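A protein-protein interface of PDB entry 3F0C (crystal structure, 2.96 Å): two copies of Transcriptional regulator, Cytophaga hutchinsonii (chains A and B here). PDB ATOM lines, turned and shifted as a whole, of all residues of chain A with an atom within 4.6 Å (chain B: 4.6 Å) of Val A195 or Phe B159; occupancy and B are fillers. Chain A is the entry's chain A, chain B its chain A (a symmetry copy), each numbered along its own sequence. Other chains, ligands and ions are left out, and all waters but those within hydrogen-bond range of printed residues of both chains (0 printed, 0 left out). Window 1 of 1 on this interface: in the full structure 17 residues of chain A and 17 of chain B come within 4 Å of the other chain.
OE2 of Glu B155 is in salt-bridge range of NZ of Lys A194, at 3.8 Å.
CE1 of Phe B159 touches OD1 of Asn A191, 3.5 Å away.
OD1 of Asn B156 touches NZ of Lys A194, at 3.9 Å.
Lys A194 touches Phe B159.
CZ of Phe B159 touches CG2 of Val A195, 3.5 Å away.
Met A198 touches Phe B159.
Met A198 touches Phe B199 (CE to N, 2.9 Å).
Val A195 touches just one residue of chain B: Phe B159 (3.5 Å).
Of the printed residues of chain B, Met A198 touches Phe B159 and Phe B199.
Of the printed residues of chain A, Glu B155 touches Lys A194.
Phe B159 touches just these residues of chain A: Asn A191 (3.5 Å), Lys A194 (3.5 Å), Val A195 (3.5 Å) and Met A198 (3.9 Å).
The nearest printed residue of chain A that does not touch Phe B159 is Val A167 (5.2 Å).
The nearest printed residue of chain B that does not touch Lys A194 is Phe B199 (6.3 Å).
3 positions are printed for both chains.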
ATOM      1  N   LEU A 160     -25.428   9.919 -12.734  1.00  0.00           N
ATOM      2  CA  LEU A 160     -25.953  10.802 -13.749  1.00  0.00           C
ATOM      3  C   LEU A 160     -27.464  10.904 -13.615  1.00  0.00           C
ATOM      4  O   LEU A 160     -28.025  12.003 -13.609  1.00  0.00           O
ATOM      5  CB  LEU A 160     -25.562  10.328 -15.148  1.00  0.00           C
ATOM      6  CG  LEU A 160     -25.838  11.325 -16.266  1.00  0.00           C
ATOM      7  CD1 LEU A 160     -27.271  11.332 -16.569  1.00  0.00           C
ATOM      8  CD2 LEU A 160     -25.461  12.694 -15.848  1.00  0.00           C
ATOM      9  N   LEU A 163     -28.269  12.929 -10.585  1.00  0.00           N
ATOM     10  CA  LEU A 163     -27.861  14.278 -10.787  1.00  0.00           C
ATOM     11  C   LEU A 163     -28.969  14.974 -11.523  1.00  0.00           C
ATOM     12  O   LEU A 163     -29.407  16.049 -11.099  1.00  0.00           O
ATOM     13  CB  LEU A 163     -26.593  14.340 -11.613  1.00  0.00           C
ATOM     14  CG  LEU A 163     -25.338  14.221 -10.759  1.00  0.00           C
ATOM     15  CD1 LEU A 163     -24.113  14.064 -11.684  1.00  0.00           C
ATOM     16  CD2 LEU A 163     -25.222  15.412  -9.809  1.00  0.00           C
ATOM     17  N   LEU A 164     -29.460  14.375 -12.607  1.00  0.00           N
ATOM     18  CA  LEU A 164     -30.519  15.032 -13.382  1.00  0.00           C
ATOM     19  C   LEU A 164     -31.778  15.151 -12.540  1.00  0.00           C
ATOM     20  O   LEU A 164     -32.442  16.177 -12.529  1.00  0.00           O
ATOM     21  CB  LEU A 164     -30.842  14.269 -14.637  1.00  0.00           C
ATOM     22  CG  LEU A 164     -29.626  13.969 -15.501  1.00  0.00           C
ATOM     23  CD1 LEU A 164     -30.063  13.085 -16.682  1.00  0.00           C
ATOM     24  CD2 LEU A 164     -28.891  15.277 -15.919  1.00  0.00           C
ATOM     25  N   VAL A 167     -31.690  18.229 -10.354  1.00  0.00           N
ATOM     26  CA  VAL A 167     -31.966  19.460 -11.056  1.00  0.00           C
ATOM     27  C   VAL A 167     -33.481  19.657 -11.095  1.00  0.00           C
ATOM     28  O   VAL A 167     -34.004  20.715 -10.790  1.00  0.00           O
ATOM     29  CB  VAL A 167     -31.401  19.449 -12.468  1.00  0.00           C
ATOM     30  CG1 VAL A 167     -32.076  20.568 -13.302  1.00  0.00           C
ATOM     31  CG2 VAL A 167     -29.873  19.595 -12.439  1.00  0.00           C
ATOM     32  N   ASN A 191     -29.439  23.691 -17.243  1.00  0.00           N
ATOM     33  CA  ASN A 191     -28.802  23.030 -16.100  1.00  0.00           C
ATOM     34  C   ASN A 191     -28.457  21.557 -16.293  1.00  0.00           C
ATOM     35  O   ASN A 191     -27.355  21.115 -15.962  1.00  0.00           O
ATOM     36  CB  ASN A 191     -29.746  23.075 -14.921  1.00  0.00           C
ATOM     37  CG  ASN A 191     -29.766  24.390 -14.266  1.00  0.00           C
ATOM     38  OD1 ASN A 191     -28.711  24.907 -13.906  1.00  0.00           O
ATOM     39  ND2 ASN A 191     -30.971  24.947 -14.074  1.00  0.00           N
ATOM     40  N   MET A 192     -29.432  20.792 -16.778  1.00  0.00           N
ATOM     41  CA  MET A 192     -29.220  19.384 -17.057  1.00  0.00           C
ATOM     42  C   MET A 192     -28.058  19.112 -18.009  1.00  0.00           C
ATOM     43  O   MET A 192     -27.455  18.074 -17.922  1.00  0.00           O
ATOM     44  CB  MET A 192     -30.510  18.705 -17.515  1.00  0.00           C
ATOM     45  CG  MET A 192     -31.400  18.308 -16.330  1.00  0.00           C
ATOM     46  SD  MET A 192     -33.163  17.448 -16.731  1.00  0.00           S
ATOM     47  CE  MET A 192     -32.614  15.655 -17.454  1.00  0.00           C
ATOM     48  N   CYS A 193     -27.730  20.071 -18.869  1.00  0.00           N
ATOM     49  CA  CYS A 193     -26.551  19.950 -19.720  1.00  0.00           C
ATOM     50  C   CYS A 193     -25.286  20.129 -18.881  1.00  0.00           C
ATOM     51  O   CYS A 193     -24.436  19.241 -18.815  1.00  0.00           O
ATOM     52  CB  CYS A 193     -26.591  20.984 -20.845  1.00  0.00           C
ATOM     53  SG  CYS A 193     -28.083  20.922 -21.864  1.00  0.00           S
ATOM     54  N   LYS A 194     -25.178  21.289 -18.239  1.00  0.00           N
ATOM     55  CA  LYS A 194     -24.090  21.597 -17.355  1.00  0.00           C
ATOM     56  C   LYS A 194     -23.698  20.290 -16.659  1.00  0.00           C
ATOM     57  O   LYS A 194     -22.554  19.851 -16.737  1.00  0.00           O
ATOM     58  CB  LYS A 194     -24.529  22.633 -16.328  1.00  0.00           C
ATOM     59  CG  LYS A 194     -24.460  24.067 -16.774  1.00  0.00           C
ATOM     60  CD  LYS A 194     -24.190  25.022 -15.578  1.00  0.00           C
ATOM     61  CE  LYS A 194     -22.971  25.874 -15.824  1.00  0.00           C
ATOM     62  NZ  LYS A 194     -22.910  26.912 -14.812  1.00  0.00           N
ATOM     63  N   VAL A 195     -24.679  19.655 -16.024  1.00  0.00           N
ATOM     64  CA  VAL A 195     -24.448  18.421 -15.298  1.00  0.00           C
ATOM     65  C   VAL A 195     -23.911  17.316 -16.236  1.00  0.00           C
ATOM     66  O   VAL A 195     -22.814  16.796 -16.006  1.00  0.00           O
ATOM     67  CB  VAL A 195     -25.739  17.979 -14.578  1.00  0.00           C
ATOM     68  CG1 VAL A 195     -25.528  16.644 -13.829  1.00  0.00           C
ATOM     69  CG2 VAL A 195     -26.226  19.080 -13.640  1.00  0.00           C
ATOM     70  N   ALA A 196     -24.677  16.987 -17.286  1.00  0.00           N
ATOM     71  CA  ALA A 196     -24.225  16.140 -18.415  1.00  0.00           C
ATOM     72  C   ALA A 196     -22.776  16.431 -18.855  1.00  0.00           C
ATOM     73  O   ALA A 196     -21.892  15.558 -18.846  1.00  0.00           O
ATOM     74  CB  ALA A 196     -25.150  16.341 -19.594  1.00  0.00           C
ATOM     75  N   GLY A 197     -22.527  17.671 -19.236  1.00  0.00           N
ATOM     76  CA  GLY A 197     -21.189  18.080 -19.570  1.00  0.00           C
ATOM     77  C   GLY A 197     -20.139  17.705 -18.546  1.00  0.00           C
ATOM     78  O   GLY A 197     -19.073  17.197 -18.889  1.00  0.00           O
ATOM     79  N   MET A 198     -20.431  17.953 -17.284  1.00  0.00           N
ATOM     80  CA  MET A 198     -19.449  17.702 -16.248  1.00  0.00           C
ATOM     81  C   MET A 198     -19.228  16.215 -16.026  1.00  0.00           C
ATOM     82  O   MET A 198     -18.102  15.748 -15.837  1.00  0.00           O
ATOM     83  CB  MET A 198     -19.920  18.305 -14.959  1.00  0.00           C
ATOM     84  CG  MET A 198     -20.113  19.796 -14.993  1.00  0.00           C
ATOM     85  SD  MET A 198     -20.594  20.357 -13.190  1.00  0.00           S
ATOM     86  CE  MET A 198     -18.876  19.967 -12.335  1.00  0.00           C
ATOM     87  N   PHE A 199     -20.326  15.475 -16.031  1.00  0.00           N
ATOM     88  CA  PHE A 199     -20.280  14.032 -15.896  1.00  0.00           C
ATOM     89  C   PHE A 199     -19.390  13.429 -16.975  1.00  0.00           C
ATOM     90  O   PHE A 199     -18.546  12.566 -16.690  1.00  0.00           O
ATOM     91  CB  PHE A 199     -21.695  13.479 -15.983  1.00  0.00           C
ATOM     92  CG  PHE A 199     -21.787  12.012 -15.765  1.00  0.00           C
ATOM     93  CD1 PHE A 199     -21.937  11.151 -16.848  1.00  0.00           C
ATOM     94  CD2 PHE A 199     -21.762  11.488 -14.484  1.00  0.00           C
ATOM     95  CE1 PHE A 199     -22.048   9.790 -16.658  1.00  0.00           C
ATOM     96  CE2 PHE A 199     -21.873  10.110 -14.277  1.00  0.00           C
ATOM     97  CZ  PHE A 199     -22.015   9.263 -15.371  1.00  0.00           C
ATOM     98  N   GLU B 155     -23.540  32.644 -10.752  1.00  0.00           N
ATOM     99  CA  GLU B 155     -24.190  31.518 -11.407  1.00  0.00           C
ATOM    100  C   GLU B 155     -23.626  30.215 -10.876  1.00  0.00           C
ATOM    101  O   GLU B 155     -24.357  29.352 -10.413  1.00  0.00           O
ATOM    102  CB  GLU B 155     -23.931  31.626 -12.898  1.00  0.00           C
ATOM    103  CG  GLU B 155     -24.589  30.581 -13.745  1.00  0.00           C
ATOM    104  CD  GLU B 155     -24.303  30.812 -15.221  1.00  0.00           C
ATOM    105  OE1 GLU B 155     -23.561  31.768 -15.566  1.00  0.00           O
ATOM    106  OE2 GLU B 155     -24.804  30.007 -16.034  1.00  0.00           O
ATOM    107  N   ASN B 156     -22.313  30.088 -10.938  1.00  0.00           N
ATOM    108  CA  ASN B 156     -21.627  28.948 -10.380  1.00  0.00           C
ATOM    109  C   ASN B 156     -22.030  28.663  -8.937  1.00  0.00           C
ATOM    110  O   ASN B 156     -22.465  27.564  -8.616  1.00  0.00           O
ATOM    111  CB  ASN B 156     -20.134  29.218 -10.430  1.00  0.00           C
ATOM    112  CG  ASN B 156     -19.577  29.143 -11.831  1.00  0.00           C
ATOM    113  OD1 ASN B 156     -20.339  29.133 -12.800  1.00  0.00           O
ATOM    114  ND2 ASN B 156     -18.243  29.079 -11.948  1.00  0.00           N
ATOM    115  N   ALA B 157     -21.885  29.668  -8.079  1.00  0.00           N
ATOM    116  CA  ALA B 157     -22.220  29.576  -6.665  1.00  0.00           C
ATOM    117  C   ALA B 157     -23.555  28.869  -6.438  1.00  0.00           C
ATOM    118  O   ALA B 157     -23.623  27.878  -5.717  1.00  0.00           O
ATOM    119  CB  ALA B 157     -22.269  30.949  -6.079  1.00  0.00           C
ATOM    120  N   GLU B 158     -24.614  29.403  -7.049  1.00  0.00           N
ATOM    121  CA  GLU B 158     -25.932  28.784  -7.093  1.00  0.00           C
ATOM    122  C   GLU B 158     -25.912  27.366  -7.540  1.00  0.00           C
ATOM    123  O   GLU B 158     -26.652  26.515  -7.020  1.00  0.00           O
ATOM    124  CB  GLU B 158     -26.747  29.448  -8.144  1.00  0.00           C
ATOM    125  CG  GLU B 158     -27.498  30.561  -7.647  1.00  0.00           C
ATOM    126  CD  GLU B 158     -28.967  30.436  -8.017  1.00  0.00           C
ATOM    127  OE1 GLU B 158     -29.283  29.918  -9.137  1.00  0.00           O
ATOM    128  OE2 GLU B 158     -29.795  30.882  -7.171  1.00  0.00           O
ATOM    129  N   PHE B 159     -25.126  27.126  -8.577  1.00  0.00           N
ATOM    130  CA  PHE B 159     -25.107  25.802  -9.163  1.00  0.00           C
ATOM    131  C   PHE B 159     -24.587  24.805  -8.143  1.00  0.00           C
ATOM    132  O   PHE B 159     -25.225  23.784  -7.882  1.00  0.00           O
ATOM    133  CB  PHE B 159     -24.291  25.771 -10.457  1.00  0.00           C
ATOM    134  CG  PHE B 159     -24.534  24.544 -11.304  1.00  0.00           C
ATOM    135  CD1 PHE B 159     -25.822  24.195 -11.702  1.00  0.00           C
ATOM    136  CD2 PHE B 159     -23.470  23.741 -11.711  1.00  0.00           C
ATOM    137  CE1 PHE B 159     -26.042  23.087 -12.498  1.00  0.00           C
ATOM    138  CE2 PHE B 159     -23.682  22.645 -12.490  1.00  0.00           C
ATOM    139  CZ  PHE B 159     -24.975  22.310 -12.885  1.00  0.00           C
ATOM    140  N   LEU B 160     -23.454  25.125  -7.546  1.00  0.00           N
ATOM    141  CA  LEU B 160     -22.897  24.243  -6.547  1.00  0.00           C
ATOM    142  C   LEU B 160     -23.899  24.038  -5.421  1.00  0.00           C
ATOM    143  O   LEU B 160     -24.166  22.905  -5.013  1.00  0.00           O
ATOM    144  CB  LEU B 160     -21.576  24.787  -6.006  1.00  0.00           C
ATOM    145  CG  LEU B 160     -20.780  23.811  -5.148  1.00  0.00           C
ATOM    146  CD1 LEU B 160     -21.392  23.721  -3.821  1.00  0.00           C
ATOM    147  CD2 LEU B 160     -20.800  22.457  -5.745  1.00  0.00           C
ATOM    148  N   VAL B 161     -24.481  25.131  -4.951  1.00  0.00           N
ATOM    149  CA  VAL B 161     -25.403  25.032  -3.832  1.00  0.00           C
ATOM    150  C   VAL B 161     -26.571  24.118  -4.244  1.00  0.00           C
ATOM    151  O   VAL B 161     -26.851  23.136  -3.571  1.00  0.00           O
ATOM    152  CB  VAL B 161     -25.794  26.416  -3.289  1.00  0.00           C
ATOM    153  CG1 VAL B 161     -26.807  26.311  -2.203  1.00  0.00           C
ATOM    154  CG2 VAL B 161     -24.567  27.079  -2.744  1.00  0.00           C
ATOM    155  N   HIS B 162     -27.175  24.378  -5.394  1.00  0.00           N
ATOM    156  CA  HIS B 162     -28.268  23.541  -5.882  1.00  0.00           C
ATOM    157  C   HIS B 162     -27.871  22.061  -6.128  1.00  0.00           C
ATOM    158  O   HIS B 162     -28.655  21.132  -5.881  1.00  0.00           O
ATOM    159  CB  HIS B 162     -28.829  24.124  -7.167  1.00  0.00           C
ATOM    160  CG  HIS B 162     -29.594  25.386  -6.969  1.00  0.00           C
ATOM    161  ND1 HIS B 162     -29.959  25.853  -5.723  1.00  0.00           N
ATOM    162  CD2 HIS B 162     -30.094  26.270  -7.867  1.00  0.00           C
ATOM    163  CE1 HIS B 162     -30.638  26.977  -5.860  1.00  0.00           C
ATOM    164  NE2 HIS B 162     -30.731  27.254  -7.150  1.00  0.00           N
ATOM    165  N   LEU B 163     -26.670  21.866  -6.661  1.00  0.00           N
ATOM    166  CA  LEU B 163     -26.176  20.554  -6.910  1.00  0.00           C
ATOM    167  C   LEU B 163     -26.203  19.810  -5.606  1.00  0.00           C
ATOM    168  O   LEU B 163     -26.733  18.696  -5.545  1.00  0.00           O
ATOM    169  CB  LEU B 163     -24.755  20.602  -7.431  1.00  0.00           C
ATOM    170  CG  LEU B 163     -24.698  20.774  -8.943  1.00  0.00           C
ATOM    171  CD1 LEU B 163     -23.238  21.043  -9.364  1.00  0.00           C
ATOM    172  CD2 LEU B 163     -25.310  19.563  -9.645  1.00  0.00           C
ATOM    173  N   PHE B 199     -17.408  20.027  -9.835  1.00  0.00           N
ATOM    174  CA  PHE B 199     -17.584  21.465  -9.905  1.00  0.00           C
ATOM    175  C   PHE B 199     -16.229  22.160  -9.950  1.00  0.00           C
ATOM    176  O   PHE B 199     -16.011  23.066 -10.768  1.00  0.00           O
ATOM    177  CB  PHE B 199     -18.394  21.926  -8.703  1.00  0.00           C
ATOM    178  CG  PHE B 199     -18.720  23.376  -8.711  1.00  0.00           C
ATOM    179  CD1 PHE B 199     -18.000  24.261  -7.915  1.00  0.00           C
ATOM    180  CD2 PHE B 199     -19.765  23.858  -9.482  1.00  0.00           C
ATOM    181  CE1 PHE B 199     -18.307  25.604  -7.895  1.00  0.00           C
ATOM    182  CE2 PHE B 199     -20.086  25.218  -9.471  1.00  0.00           C
ATOM    183  CZ  PHE B 199     -19.352  26.090  -8.674  1.00  0.00           C
